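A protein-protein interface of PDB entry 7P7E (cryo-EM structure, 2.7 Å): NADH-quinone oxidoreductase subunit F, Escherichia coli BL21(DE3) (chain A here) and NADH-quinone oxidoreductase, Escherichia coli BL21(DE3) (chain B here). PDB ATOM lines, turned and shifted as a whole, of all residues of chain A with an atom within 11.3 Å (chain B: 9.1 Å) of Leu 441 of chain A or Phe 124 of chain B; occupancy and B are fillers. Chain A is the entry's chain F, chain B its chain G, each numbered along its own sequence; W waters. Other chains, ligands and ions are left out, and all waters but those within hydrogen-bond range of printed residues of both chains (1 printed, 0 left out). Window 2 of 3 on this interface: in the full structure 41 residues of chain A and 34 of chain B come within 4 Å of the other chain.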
ATOM      1  N   TRP A 363       6.663  28.696 -13.245  1.00  0.00           N
ATOM      2  CA  TRP A 363       5.795  28.204 -12.178  1.00  0.00           C
ATOM      3  C   TRP A 363       4.501  27.635 -12.746  1.00  0.00           C
ATOM      4  O   TRP A 363       4.062  26.549 -12.345  1.00  0.00           O
ATOM      5  CB  TRP A 363       5.503  29.327 -11.181  1.00  0.00           C
ATOM      6  CG  TRP A 363       4.963  28.874  -9.845  1.00  0.00           C
ATOM      7  CD1 TRP A 363       4.581  27.613  -9.493  1.00  0.00           C
ATOM      8  CD2 TRP A 363       4.750  29.691  -8.688  1.00  0.00           C
ATOM      9  NE1 TRP A 363       4.142  27.593  -8.196  1.00  0.00           N
ATOM     10  CE2 TRP A 363       4.236  28.856  -7.677  1.00  0.00           C
ATOM     11  CE3 TRP A 363       4.945  31.045  -8.407  1.00  0.00           C
ATOM     12  CZ2 TRP A 363       3.914  29.331  -6.410  1.00  0.00           C
ATOM     13  CZ3 TRP A 363       4.625  31.514  -7.150  1.00  0.00           C
ATOM     14  CH2 TRP A 363       4.116  30.659  -6.166  1.00  0.00           C
ATOM     15  N   GLN A 377      -2.100  19.645  -6.607  1.00  0.00           N
ATOM     16  CA  GLN A 377      -2.394  19.861  -5.200  1.00  0.00           C
ATOM     17  C   GLN A 377      -3.332  21.048  -5.073  1.00  0.00           C
ATOM     18  O   GLN A 377      -3.424  21.869  -5.992  1.00  0.00           O
ATOM     19  CB  GLN A 377      -1.097  20.097  -4.409  1.00  0.00           C
ATOM     20  CG  GLN A 377      -0.196  18.873  -4.377  1.00  0.00           C
ATOM     21  CD  GLN A 377       1.062  19.076  -3.567  1.00  0.00           C
ATOM     22  OE1 GLN A 377       1.265  20.130  -2.971  1.00  0.00           O
ATOM     23  NE2 GLN A 377       1.919  18.066  -3.546  1.00  0.00           N
ATOM     24  N   PRO A 378      -4.091  21.136  -3.974  1.00  0.00           N
ATOM     25  CA  PRO A 378      -4.992  22.284  -3.792  1.00  0.00           C
ATOM     26  C   PRO A 378      -4.241  23.607  -3.756  1.00  0.00           C
ATOM     27  O   PRO A 378      -3.144  23.711  -3.204  1.00  0.00           O
ATOM     28  CB  PRO A 378      -5.668  21.989  -2.449  1.00  0.00           C
ATOM     29  CG  PRO A 378      -5.634  20.518  -2.338  1.00  0.00           C
ATOM     30  CD  PRO A 378      -4.353  20.081  -2.978  1.00  0.00           C
ATOM     31  N   GLY A 379      -4.853  24.627  -4.357  1.00  0.00           N
ATOM     32  CA  GLY A 379      -4.223  25.914  -4.534  1.00  0.00           C
ATOM     33  C   GLY A 379      -3.494  26.094  -5.849  1.00  0.00           C
ATOM     34  O   GLY A 379      -3.010  27.199  -6.120  1.00  0.00           O
ATOM     35  N   THR A 383      -3.312  29.524  -7.884  1.00  0.00           N
ATOM     36  CA  THR A 383      -2.013  30.076  -8.262  1.00  0.00           C
ATOM     37  C   THR A 383      -1.972  30.428  -9.744  1.00  0.00           C
ATOM     38  O   THR A 383      -1.412  31.462 -10.124  1.00  0.00           O
ATOM     39  CB  THR A 383      -0.903  29.087  -7.914  1.00  0.00           C
ATOM     40  OG1 THR A 383      -1.068  28.645  -6.562  1.00  0.00           O
ATOM     41  CG2 THR A 383       0.461  29.736  -8.058  1.00  0.00           C
ATOM     42  N   GLN A 386      -3.986  33.628 -10.156  1.00  0.00           N
ATOM     43  CA  GLN A 386      -3.174  34.744  -9.685  1.00  0.00           C
ATOM     44  C   GLN A 386      -2.085  35.101 -10.691  1.00  0.00           C
ATOM     45  O   GLN A 386      -1.774  36.282 -10.888  1.00  0.00           O
ATOM     46  CB  GLN A 386      -2.563  34.399  -8.328  1.00  0.00           C
ATOM     47  CG  GLN A 386      -2.261  35.596  -7.453  1.00  0.00           C
ATOM     48  CD  GLN A 386      -1.042  35.382  -6.582  1.00  0.00           C
ATOM     49  OE1 GLN A 386       0.043  35.882  -6.879  1.00  0.00           O
ATOM     50  NE2 GLN A 386      -1.216  34.642  -5.496  1.00  0.00           N
ATOM     51  N   PHE A 427      -1.989  19.040  -0.470  1.00  0.00           N
ATOM     52  CA  PHE A 427      -0.927  20.030  -0.560  1.00  0.00           C
ATOM     53  C   PHE A 427       0.145  19.775   0.490  1.00  0.00           C
ATOM     54  O   PHE A 427      -0.161  19.587   1.672  1.00  0.00           O
ATOM     55  CB  PHE A 427      -1.490  21.439  -0.395  1.00  0.00           C
ATOM     56  CG  PHE A 427      -0.432  22.501  -0.308  1.00  0.00           C
ATOM     57  CD1 PHE A 427       0.402  22.753  -1.385  1.00  0.00           C
ATOM     58  CD2 PHE A 427      -0.262  23.236   0.853  1.00  0.00           C
ATOM     59  CE1 PHE A 427       1.383  23.723  -1.308  1.00  0.00           C
ATOM     60  CE2 PHE A 427       0.717  24.208   0.935  1.00  0.00           C
ATOM     61  CZ  PHE A 427       1.540  24.452  -0.147  1.00  0.00           C
ATOM     62  N   SER A 428       1.403  19.782   0.056  1.00  0.00           N
ATOM     63  CA  SER A 428       2.529  19.597   0.961  1.00  0.00           C
ATOM     64  C   SER A 428       3.789  20.142   0.309  1.00  0.00           C
ATOM     65  O   SER A 428       4.084  19.812  -0.843  1.00  0.00           O
ATOM     66  CB  SER A 428       2.719  18.119   1.317  1.00  0.00           C
ATOM     67  OG  SER A 428       3.881  17.930   2.105  1.00  0.00           O
ATOM     68  N   ASN A 429       4.525  20.978   1.045  1.00  0.00           N
ATOM     69  CA  ASN A 429       5.877  21.344   0.642  1.00  0.00           C
ATOM     70  C   ASN A 429       6.831  21.335   1.832  1.00  0.00           C
ATOM     71  O   ASN A 429       7.915  21.925   1.751  1.00  0.00           O
ATOM     72  CB  ASN A 429       5.908  22.711  -0.058  1.00  0.00           C
ATOM     73  CG  ASN A 429       5.558  23.861   0.866  1.00  0.00           C
ATOM     74  OD1 ASN A 429       4.868  23.689   1.870  1.00  0.00           O
ATOM     75  ND2 ASN A 429       6.035  25.050   0.523  1.00  0.00           N
ATOM     76  N   THR A 430       6.455  20.685   2.928  1.00  0.00           N
ATOM     77  CA  THR A 430       7.271  20.597   4.130  1.00  0.00           C
ATOM     78  C   THR A 430       7.518  19.136   4.470  1.00  0.00           C
ATOM     79  O   THR A 430       6.573  18.345   4.544  1.00  0.00           O
ATOM     80  CB  THR A 430       6.594  21.289   5.316  1.00  0.00           C
ATOM     81  OG1 THR A 430       5.189  21.013   5.293  1.00  0.00           O
ATOM     82  CG2 THR A 430       6.810  22.783   5.264  1.00  0.00           C
ATOM     83  N   GLN A 437       7.842  20.174  16.489  1.00  0.00           N
ATOM     84  CA  GLN A 437       6.408  20.074  16.251  1.00  0.00           C
ATOM     85  C   GLN A 437       5.979  21.143  15.253  1.00  0.00           C
ATOM     86  O   GLN A 437       6.308  22.318  15.435  1.00  0.00           O
ATOM     87  CB  GLN A 437       5.633  20.225  17.553  1.00  0.00           C
ATOM     88  CG  GLN A 437       5.839  19.077  18.526  1.00  0.00           C
ATOM     89  CD  GLN A 437       5.201  19.335  19.874  1.00  0.00           C
ATOM     90  OE1 GLN A 437       5.653  20.188  20.634  1.00  0.00           O
ATOM     91  NE2 GLN A 437       4.142  18.597  20.178  1.00  0.00           N
ATOM     92  N   PRO A 438       5.266  20.776  14.191  1.00  0.00           N
ATOM     93  CA  PRO A 438       4.878  21.768  13.184  1.00  0.00           C
ATOM     94  C   PRO A 438       3.794  22.707  13.689  1.00  0.00           C
ATOM     95  O   PRO A 438       3.075  22.426  14.650  1.00  0.00           O
ATOM     96  CB  PRO A 438       4.367  20.910  12.023  1.00  0.00           C
ATOM     97  CG  PRO A 438       3.908  19.652  12.670  1.00  0.00           C
ATOM     98  CD  PRO A 438       4.835  19.417  13.825  1.00  0.00           C
ATOM     99  N   ASN A 439       3.694  23.852  13.015  1.00  0.00           N
ATOM    100  CA  ASN A 439       2.652  24.842  13.285  1.00  0.00           C
ATOM    101  C   ASN A 439       1.476  24.531  12.370  1.00  0.00           C
ATOM    102  O   ASN A 439       1.427  24.951  11.214  1.00  0.00           O
ATOM    103  CB  ASN A 439       3.183  26.253  13.066  1.00  0.00           C
ATOM    104  CG  ASN A 439       2.294  27.314  13.678  1.00  0.00           C
ATOM    105  OD1 ASN A 439       1.901  27.214  14.837  1.00  0.00           O
ATOM    106  ND2 ASN A 439       1.970  28.336  12.899  1.00  0.00           N
ATOM    107  N   LEU A 440       0.510  23.784  12.899  1.00  0.00           N
ATOM    108  CA  LEU A 440      -0.612  23.279  12.108  1.00  0.00           C
ATOM    109  C   LEU A 440      -1.598  24.412  11.861  1.00  0.00           C
ATOM    110  O   LEU A 440      -2.493  24.675  12.664  1.00  0.00           O
ATOM    111  CB  LEU A 440      -1.276  22.106  12.818  1.00  0.00           C
ATOM    112  CG  LEU A 440      -0.358  20.916  13.100  1.00  0.00           C
ATOM    113  CD1 LEU A 440      -1.034  19.921  14.028  1.00  0.00           C
ATOM    114  CD2 LEU A 440       0.057  20.251  11.798  1.00  0.00           C
ATOM    115  N   LEU A 441      -1.433  25.087  10.726  1.00  0.00           N
ATOM    116  CA  LEU A 441      -2.328  26.175  10.362  1.00  0.00           C
ATOM    117  C   LEU A 441      -3.691  25.636   9.940  1.00  0.00           C
ATOM    118  O   LEU A 441      -3.819  24.504   9.468  1.00  0.00           O
ATOM    119  CB  LEU A 441      -1.726  27.007   9.230  1.00  0.00           C
ATOM    120  CG  LEU A 441      -0.561  27.932   9.585  1.00  0.00           C
ATOM    121  CD1 LEU A 441      -0.087  28.681   8.349  1.00  0.00           C
ATOM    122  CD2 LEU A 441      -0.953  28.902  10.684  1.00  0.00           C
ATOM    123  N   LYS A 442      -4.714  26.466  10.117  1.00  0.00           N
ATOM    124  CA  LYS A 442      -6.075  26.090   9.754  1.00  0.00           C
ATOM    125  C   LYS A 442      -6.668  27.080   8.756  1.00  0.00           C
ATOM    126  O   LYS A 442      -6.033  27.429   7.761  1.00  0.00           O
ATOM    127  CB  LYS A 442      -6.960  26.006  11.000  1.00  0.00           C
ATOM    128  CG  LYS A 442      -7.168  24.593  11.520  1.00  0.00           C
ATOM    129  CD  LYS A 442      -5.929  24.079  12.230  1.00  0.00           C
ATOM    130  CE  LYS A 442      -6.108  22.643  12.691  1.00  0.00           C
ATOM    131  NZ  LYS A 442      -4.811  22.023  13.083  1.00  0.00           N
ATOM    132  N   GLU B  88       4.384  41.813  -3.366  1.00  0.00           N
ATOM    133  CA  GLU B  88       4.614  40.556  -2.662  1.00  0.00           C
ATOM    134  C   GLU B  88       4.773  39.392  -3.636  1.00  0.00           C
ATOM    135  O   GLU B  88       5.591  38.493  -3.412  1.00  0.00           O
ATOM    136  CB  GLU B  88       3.468  40.295  -1.688  1.00  0.00           C
ATOM    137  CG  GLU B  88       3.701  39.129  -0.755  1.00  0.00           C
ATOM    138  CD  GLU B  88       2.525  38.887   0.165  1.00  0.00           C
ATOM    139  OE1 GLU B  88       1.599  39.724   0.180  1.00  0.00           O
ATOM    140  OE2 GLU B  88       2.526  37.861   0.873  1.00  0.00           O
ATOM    141  N   VAL B  91       8.265  39.516  -5.107  1.00  0.00           N
ATOM    142  CA  VAL B  91       9.202  38.954  -4.133  1.00  0.00           C
ATOM    143  C   VAL B  91       9.109  37.428  -4.111  1.00  0.00           C
ATOM    144  O   VAL B  91      10.131  36.734  -4.083  1.00  0.00           O
ATOM    145  CB  VAL B  91       8.958  39.570  -2.740  1.00  0.00           C
ATOM    146  CG1 VAL B  91       9.432  38.646  -1.631  1.00  0.00           C
ATOM    147  CG2 VAL B  91       9.667  40.898  -2.627  1.00  0.00           C
ATOM    148  N   GLU B  92       7.889  36.886  -4.167  1.00  0.00           N
ATOM    149  CA  GLU B  92       7.707  35.435  -4.163  1.00  0.00           C
ATOM    150  C   GLU B  92       8.297  34.781  -5.409  1.00  0.00           C
ATOM    151  O   GLU B  92       8.926  33.714  -5.326  1.00  0.00           O
ATOM    152  CB  GLU B  92       6.223  35.101  -4.038  1.00  0.00           C
ATOM    153  CG  GLU B  92       5.934  33.621  -4.017  1.00  0.00           C
ATOM    154  CD  GLU B  92       4.504  33.310  -3.647  1.00  0.00           C
ATOM    155  OE1 GLU B  92       3.610  34.120  -3.964  1.00  0.00           O
ATOM    156  OE2 GLU B  92       4.277  32.252  -3.027  1.00  0.00           O
ATOM    157  N   TRP B  93       8.104  35.408  -6.575  1.00  0.00           N
ATOM    158  CA  TRP B  93       8.687  34.904  -7.815  1.00  0.00           C
ATOM    159  C   TRP B  93      10.206  34.898  -7.743  1.00  0.00           C
ATOM    160  O   TRP B  93      10.853  33.969  -8.237  1.00  0.00           O
ATOM    161  CB  TRP B  93       8.221  35.744  -9.001  1.00  0.00           C
ATOM    162  CG  TRP B  93       6.796  35.526  -9.388  1.00  0.00           C
ATOM    163  CD1 TRP B  93       6.116  34.348  -9.371  1.00  0.00           C
ATOM    164  CD2 TRP B  93       5.876  36.516  -9.855  1.00  0.00           C
ATOM    165  NE1 TRP B  93       4.827  34.542  -9.795  1.00  0.00           N
ATOM    166  CE2 TRP B  93       4.654  35.865 -10.098  1.00  0.00           C
ATOM    167  CE3 TRP B  93       5.967  37.889 -10.089  1.00  0.00           C
ATOM    168  CZ2 TRP B  93       3.531  36.542 -10.564  1.00  0.00           C
ATOM    169  CZ3 TRP B  93       4.852  38.558 -10.546  1.00  0.00           C
ATOM    170  CH2 TRP B  93       3.651  37.884 -10.782  1.00  0.00           C
ATOM    171  N   MET B  95      11.767  34.521  -4.936  1.00  0.00           N
ATOM    172  CA  MET B  95      12.065  33.532  -3.907  1.00  0.00           C
ATOM    173  C   MET B  95      11.913  32.092  -4.375  1.00  0.00           C
ATOM    174  O   MET B  95      12.377  31.193  -3.666  1.00  0.00           O
ATOM    175  CB  MET B  95      11.168  33.742  -2.687  1.00  0.00           C
ATOM    176  CG  MET B  95      11.577  34.909  -1.834  1.00  0.00           C
ATOM    177  SD  MET B  95      13.091  34.534  -0.959  1.00  0.00           S
ATOM    178  CE  MET B  95      14.191  35.707  -1.739  1.00  0.00           C
ATOM    179  N   THR B  96      11.261  31.851  -5.517  1.00  0.00           N
ATOM    180  CA  THR B  96      11.042  30.477  -5.969  1.00  0.00           C
ATOM    181  C   THR B  96      12.354  29.746  -6.241  1.00  0.00           C
ATOM    182  O   THR B  96      12.493  28.564  -5.909  1.00  0.00           O
ATOM    183  CB  THR B  96      10.165  30.455  -7.221  1.00  0.00           C
ATOM    184  OG1 THR B  96      10.678  31.383  -8.182  1.00  0.00           O
ATOM    185  CG2 THR B  96       8.735  30.816  -6.879  1.00  0.00           C
ATOM    186  N   THR B 117      12.233  41.404   1.006  1.00  0.00           N
ATOM    187  CA  THR B 117      11.361  40.279   1.318  1.00  0.00           C
ATOM    188  C   THR B 117      10.593  40.531   2.607  1.00  0.00           C
ATOM    189  O   THR B 117       9.387  40.270   2.682  1.00  0.00           O
ATOM    190  CB  THR B 117      12.185  38.995   1.425  1.00  0.00           C
ATOM    191  OG1 THR B 117      12.876  38.770   0.193  1.00  0.00           O
ATOM    192  CG2 THR B 117      11.294  37.802   1.721  1.00  0.00           C
ATOM    193  N   GLY B 121       6.339  41.786   3.284  1.00  0.00           N
ATOM    194  CA  GLY B 121       5.573  40.909   4.140  1.00  0.00           C
ATOM    195  C   GLY B 121       5.504  39.470   3.689  1.00  0.00           C
ATOM    196  O   GLY B 121       4.683  38.713   4.218  1.00  0.00           O
ATOM    197  N   HIS B 122       6.331  39.067   2.731  1.00  0.00           N
ATOM    198  CA  HIS B 122       6.317  37.699   2.230  1.00  0.00           C
ATOM    199  C   HIS B 122       7.145  36.806   3.146  1.00  0.00           C
ATOM    200  O   HIS B 122       8.361  36.983   3.263  1.00  0.00           O
ATOM    201  CB  HIS B 122       6.856  37.653   0.805  1.00  0.00           C
ATOM    202  CG  HIS B 122       6.953  36.271   0.240  1.00  0.00           C
ATOM    203  ND1 HIS B 122       5.846  35.530  -0.106  1.00  0.00           N
ATOM    204  CD2 HIS B 122       8.027  35.495  -0.035  1.00  0.00           C
ATOM    205  CE1 HIS B 122       6.233  34.357  -0.571  1.00  0.00           C
ATOM    206  NE2 HIS B 122       7.551  34.310  -0.539  1.00  0.00           N
ATOM    207  N   SER B 123       6.488  35.848   3.793  1.00  0.00           N
ATOM    208  CA  SER B 123       7.179  34.919   4.674  1.00  0.00           C
ATOM    209  C   SER B 123       6.710  33.479   4.532  1.00  0.00           C
ATOM    210  O   SER B 123       7.259  32.605   5.210  1.00  0.00           O
ATOM    211  CB  SER B 123       7.024  35.361   6.138  1.00  0.00           C
ATOM    212  OG  SER B 123       5.660  35.529   6.476  1.00  0.00           O
ATOM    213  N   PHE B 124       5.729  33.201   3.679  1.00  0.00           N
ATOM    214  CA  PHE B 124       5.147  31.875   3.535  1.00  0.00           C
ATOM    215  C   PHE B 124       5.434  31.350   2.136  1.00  0.00           C
ATOM    216  O   PHE B 124       5.130  32.019   1.146  1.00  0.00           O
ATOM    217  CB  PHE B 124       3.636  31.922   3.791  1.00  0.00           C
ATOM    218  CG  PHE B 124       2.995  30.572   3.914  1.00  0.00           C
ATOM    219  CD1 PHE B 124       2.969  29.912   5.130  1.00  0.00           C
ATOM    220  CD2 PHE B 124       2.401  29.967   2.816  1.00  0.00           C
ATOM    221  CE1 PHE B 124       2.375  28.672   5.249  1.00  0.00           C
ATOM    222  CE2 PHE B 124       1.807  28.727   2.928  1.00  0.00           C
ATOM    223  CZ  PHE B 124       1.793  28.080   4.146  1.00  0.00           C
ATOM    224  N   ARG B 125       6.003  30.151   2.060  1.00  0.00           N
ATOM    225  CA  ARG B 125       6.367  29.528   0.794  1.00  0.00           C
ATOM    226  C   ARG B 125       5.296  28.521   0.399  1.00  0.00           C
ATOM    227  O   ARG B 125       5.002  27.595   1.160  1.00  0.00           O
ATOM    228  CB  ARG B 125       7.728  28.840   0.902  1.00  0.00           C
ATOM    229  CG  ARG B 125       8.267  28.267  -0.400  1.00  0.00           C
ATOM    230  CD  ARG B 125       9.677  27.744  -0.203  1.00  0.00           C
ATOM    231  NE  ARG B 125      10.289  27.256  -1.433  1.00  0.00           N
ATOM    232  CZ  ARG B 125      10.923  28.019  -2.313  1.00  0.00           C
ATOM    233  NH1 ARG B 125      11.016  29.327  -2.152  1.00  0.00           N
ATOM    234  NH2 ARG B 125      11.476  27.453  -3.380  1.00  0.00           N
ATOM    235  N   ARG B 126       4.714  28.703  -0.786  1.00  0.00           N
ATOM    236  CA  ARG B 126       3.810  27.717  -1.355  1.00  0.00           C
ATOM    237  C   ARG B 126       4.337  27.114  -2.649  1.00  0.00           C
ATOM    238  O   ARG B 126       3.709  26.198  -3.190  1.00  0.00           O
ATOM    239  CB  ARG B 126       2.421  28.322  -1.592  1.00  0.00           C
ATOM    240  CG  ARG B 126       2.431  29.695  -2.206  1.00  0.00           C
ATOM    241  CD  ARG B 126       1.018  30.213  -2.389  1.00  0.00           C
ATOM    242  NE  ARG B 126       0.800  30.717  -3.739  1.00  0.00           N
ATOM    243  CZ  ARG B 126       0.977  31.978  -4.103  1.00  0.00           C
ATOM    244  NH1 ARG B 126       1.354  32.901  -3.234  1.00  0.00           N
ATOM    245  NH2 ARG B 126       0.767  32.324  -5.369  1.00  0.00           N
ATOM    246  N   TYR B 127       5.460  27.607  -3.161  1.00  0.00           N
ATOM    247  CA  TYR B 127       6.141  26.949  -4.264  1.00  0.00           C
ATOM    248  C   TYR B 127       6.777  25.656  -3.767  1.00  0.00           C
ATOM    249  O   TYR B 127       7.471  25.648  -2.747  1.00  0.00           O
ATOM    250  CB  TYR B 127       7.196  27.888  -4.850  1.00  0.00           C
ATOM    251  CG  TYR B 127       7.980  27.346  -6.022  1.00  0.00           C
ATOM    252  CD1 TYR B 127       7.493  27.451  -7.316  1.00  0.00           C
ATOM    253  CD2 TYR B 127       9.224  26.763  -5.836  1.00  0.00           C
ATOM    254  CE1 TYR B 127       8.216  26.973  -8.389  1.00  0.00           C
ATOM    255  CE2 TYR B 127       9.951  26.281  -6.900  1.00  0.00           C
ATOM    256  CZ  TYR B 127       9.442  26.389  -8.174  1.00  0.00           C
ATOM    257  OH  TYR B 127      10.169  25.908  -9.233  1.00  0.00           O
HETATM  258  O   HOH W   1       2.742  34.794  -6.801  1.00  0.00           O
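The backbone carbonyl oxygen of Arg 125 of chain B sits at hydrogen-bond distance from the side-chain amide nitrogen of Asn 429 of chain A (2.8 Å).
NE2 of Gln 386 of chain A lies close to NH2 of Arg 126 of chain B (3.1 Å).
Water W1 lies within hydrogen-bond range of the side-chain amide oxygen of Gln 386 of chain A (2.9 Å), the side-chain carboxylate of Glu 92 of chain B (3.0 Å) and the guanidinium group of Arg 126 of chain B (3.5 Å).
Of the 14 printed residues of chain B, 6 touch a printed residue of chain A.
Hydrophobic or aromatic side chains of chain B that line the printed part of chain A: Trp 93, Phe 124 and Tyr 127.
Of the 16 printed residues of chain A, 6 touch a printed residue of chain B.
Hydrophobic or aromatic side chains of chain A within 4 Å of the printed part of chain B: Trp 363, Phe 427 and Leu 441.
Among the printed residues, no Asp or Glu carboxylate lies within 4 Å of a Lys or Arg side-chain nitrogen of the other chain.
Of the printed residues of chain B, Trp 363 of chain A touches Glu 92 (3.5 Å), Trp 93 (3.6 Å), Arg 126 (3.8 Å) and Tyr 127 (3.5 Å).
Gly 379 of chain A touches none of the printed residues of chain B.
Of the printed residues of chain B, Thr 383 of chain A touches Arg 126 (3.7 Å).
Of the printed residues of chain B, Gln 386 of chain A touches Arg 126 (3.1 Å).
Of chain B, only Phe 124 comes within 4 Å of Leu 441 of chain A.
No residue of chain B comes within 4 Å of Lys 442 of chain A.
Gly 121 of chain B touches none of the printed residues of chain A.
No residue of chain A comes within 4 Å of Ser 123 of chain B.
Of chain A, only Leu 441 comes within 4 Å of Phe 124 of chain B.
Of the printed residues of chain A, Arg 125 of chain B touches Asn 429 (2.8 Å).
The nearest printed residue of chain B that does not touch Leu 441 of chain A is Arg 125 of chain B (8.9 Å).
The nearest residue of chain A that does not touch Phe 124 of chain B is Phe 427 of chain A (5.1 Å).
The nearest printed residue of chain A that does not touch Trp 93 of chain B is Gln 386 of chain A (5.1 Å).
The backbone carbonyl oxygen of Gly 379 of chain A sits at hydrogen-bond distance from the side-chain hydroxyl of Thr 383 of chain A.
OE1 of Glu 92 of chain B is in salt-bridge range of NH1 of Arg 126 of chain B.
The backbone carbonyl oxygen of Tyr 127 of chain B sits close to the guanidinium group of Arg 125 of chain B (3.5 Å).
The side-chain hydroxyl (OG1) of Thr 96 of chain B lies within hydrogen-bond range of the backbone carbonyl oxygen (O) of Trp 93 of chain B (2.6 Å).
The backbone carbonyl oxygen of Met 95 of chain B sits at hydrogen-bond distance from the guanidinium group of Arg 125 of chain B.
NH2 of Arg 125 of chain B sits at hydrogen-bond distance from O of Thr 96 of chain B, at 2.9 Å.
Glu 92 of chain B touches Trp 363 of chain A.
Trp 363 of chain A touches Trp 93 of chain B (CE3 to CD1, 3.6 Å).
CH2 of Trp 363 of chain A touches NH2 of Arg 126 of chain B, 3.8 Å away.
Tyr 127 of chain B touches Trp 363 of chain A (CD1 to NE1, 3.5 Å).
Thr 383 of chain A touches Arg 126 of chain B.
CE1 of Phe 427 of chain A touches O of Arg 126 of chain B (3.9 Å).
Arg 126 of chain B touches Asn 429 of chain A.
Asn 429 of chain A touches Tyr 127 of chain B (ND2 to O, 3.6 Å).
CE1 of Phe 124 of chain B touches CD1 of Leu 441 of chain A, at 3.96 Å.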
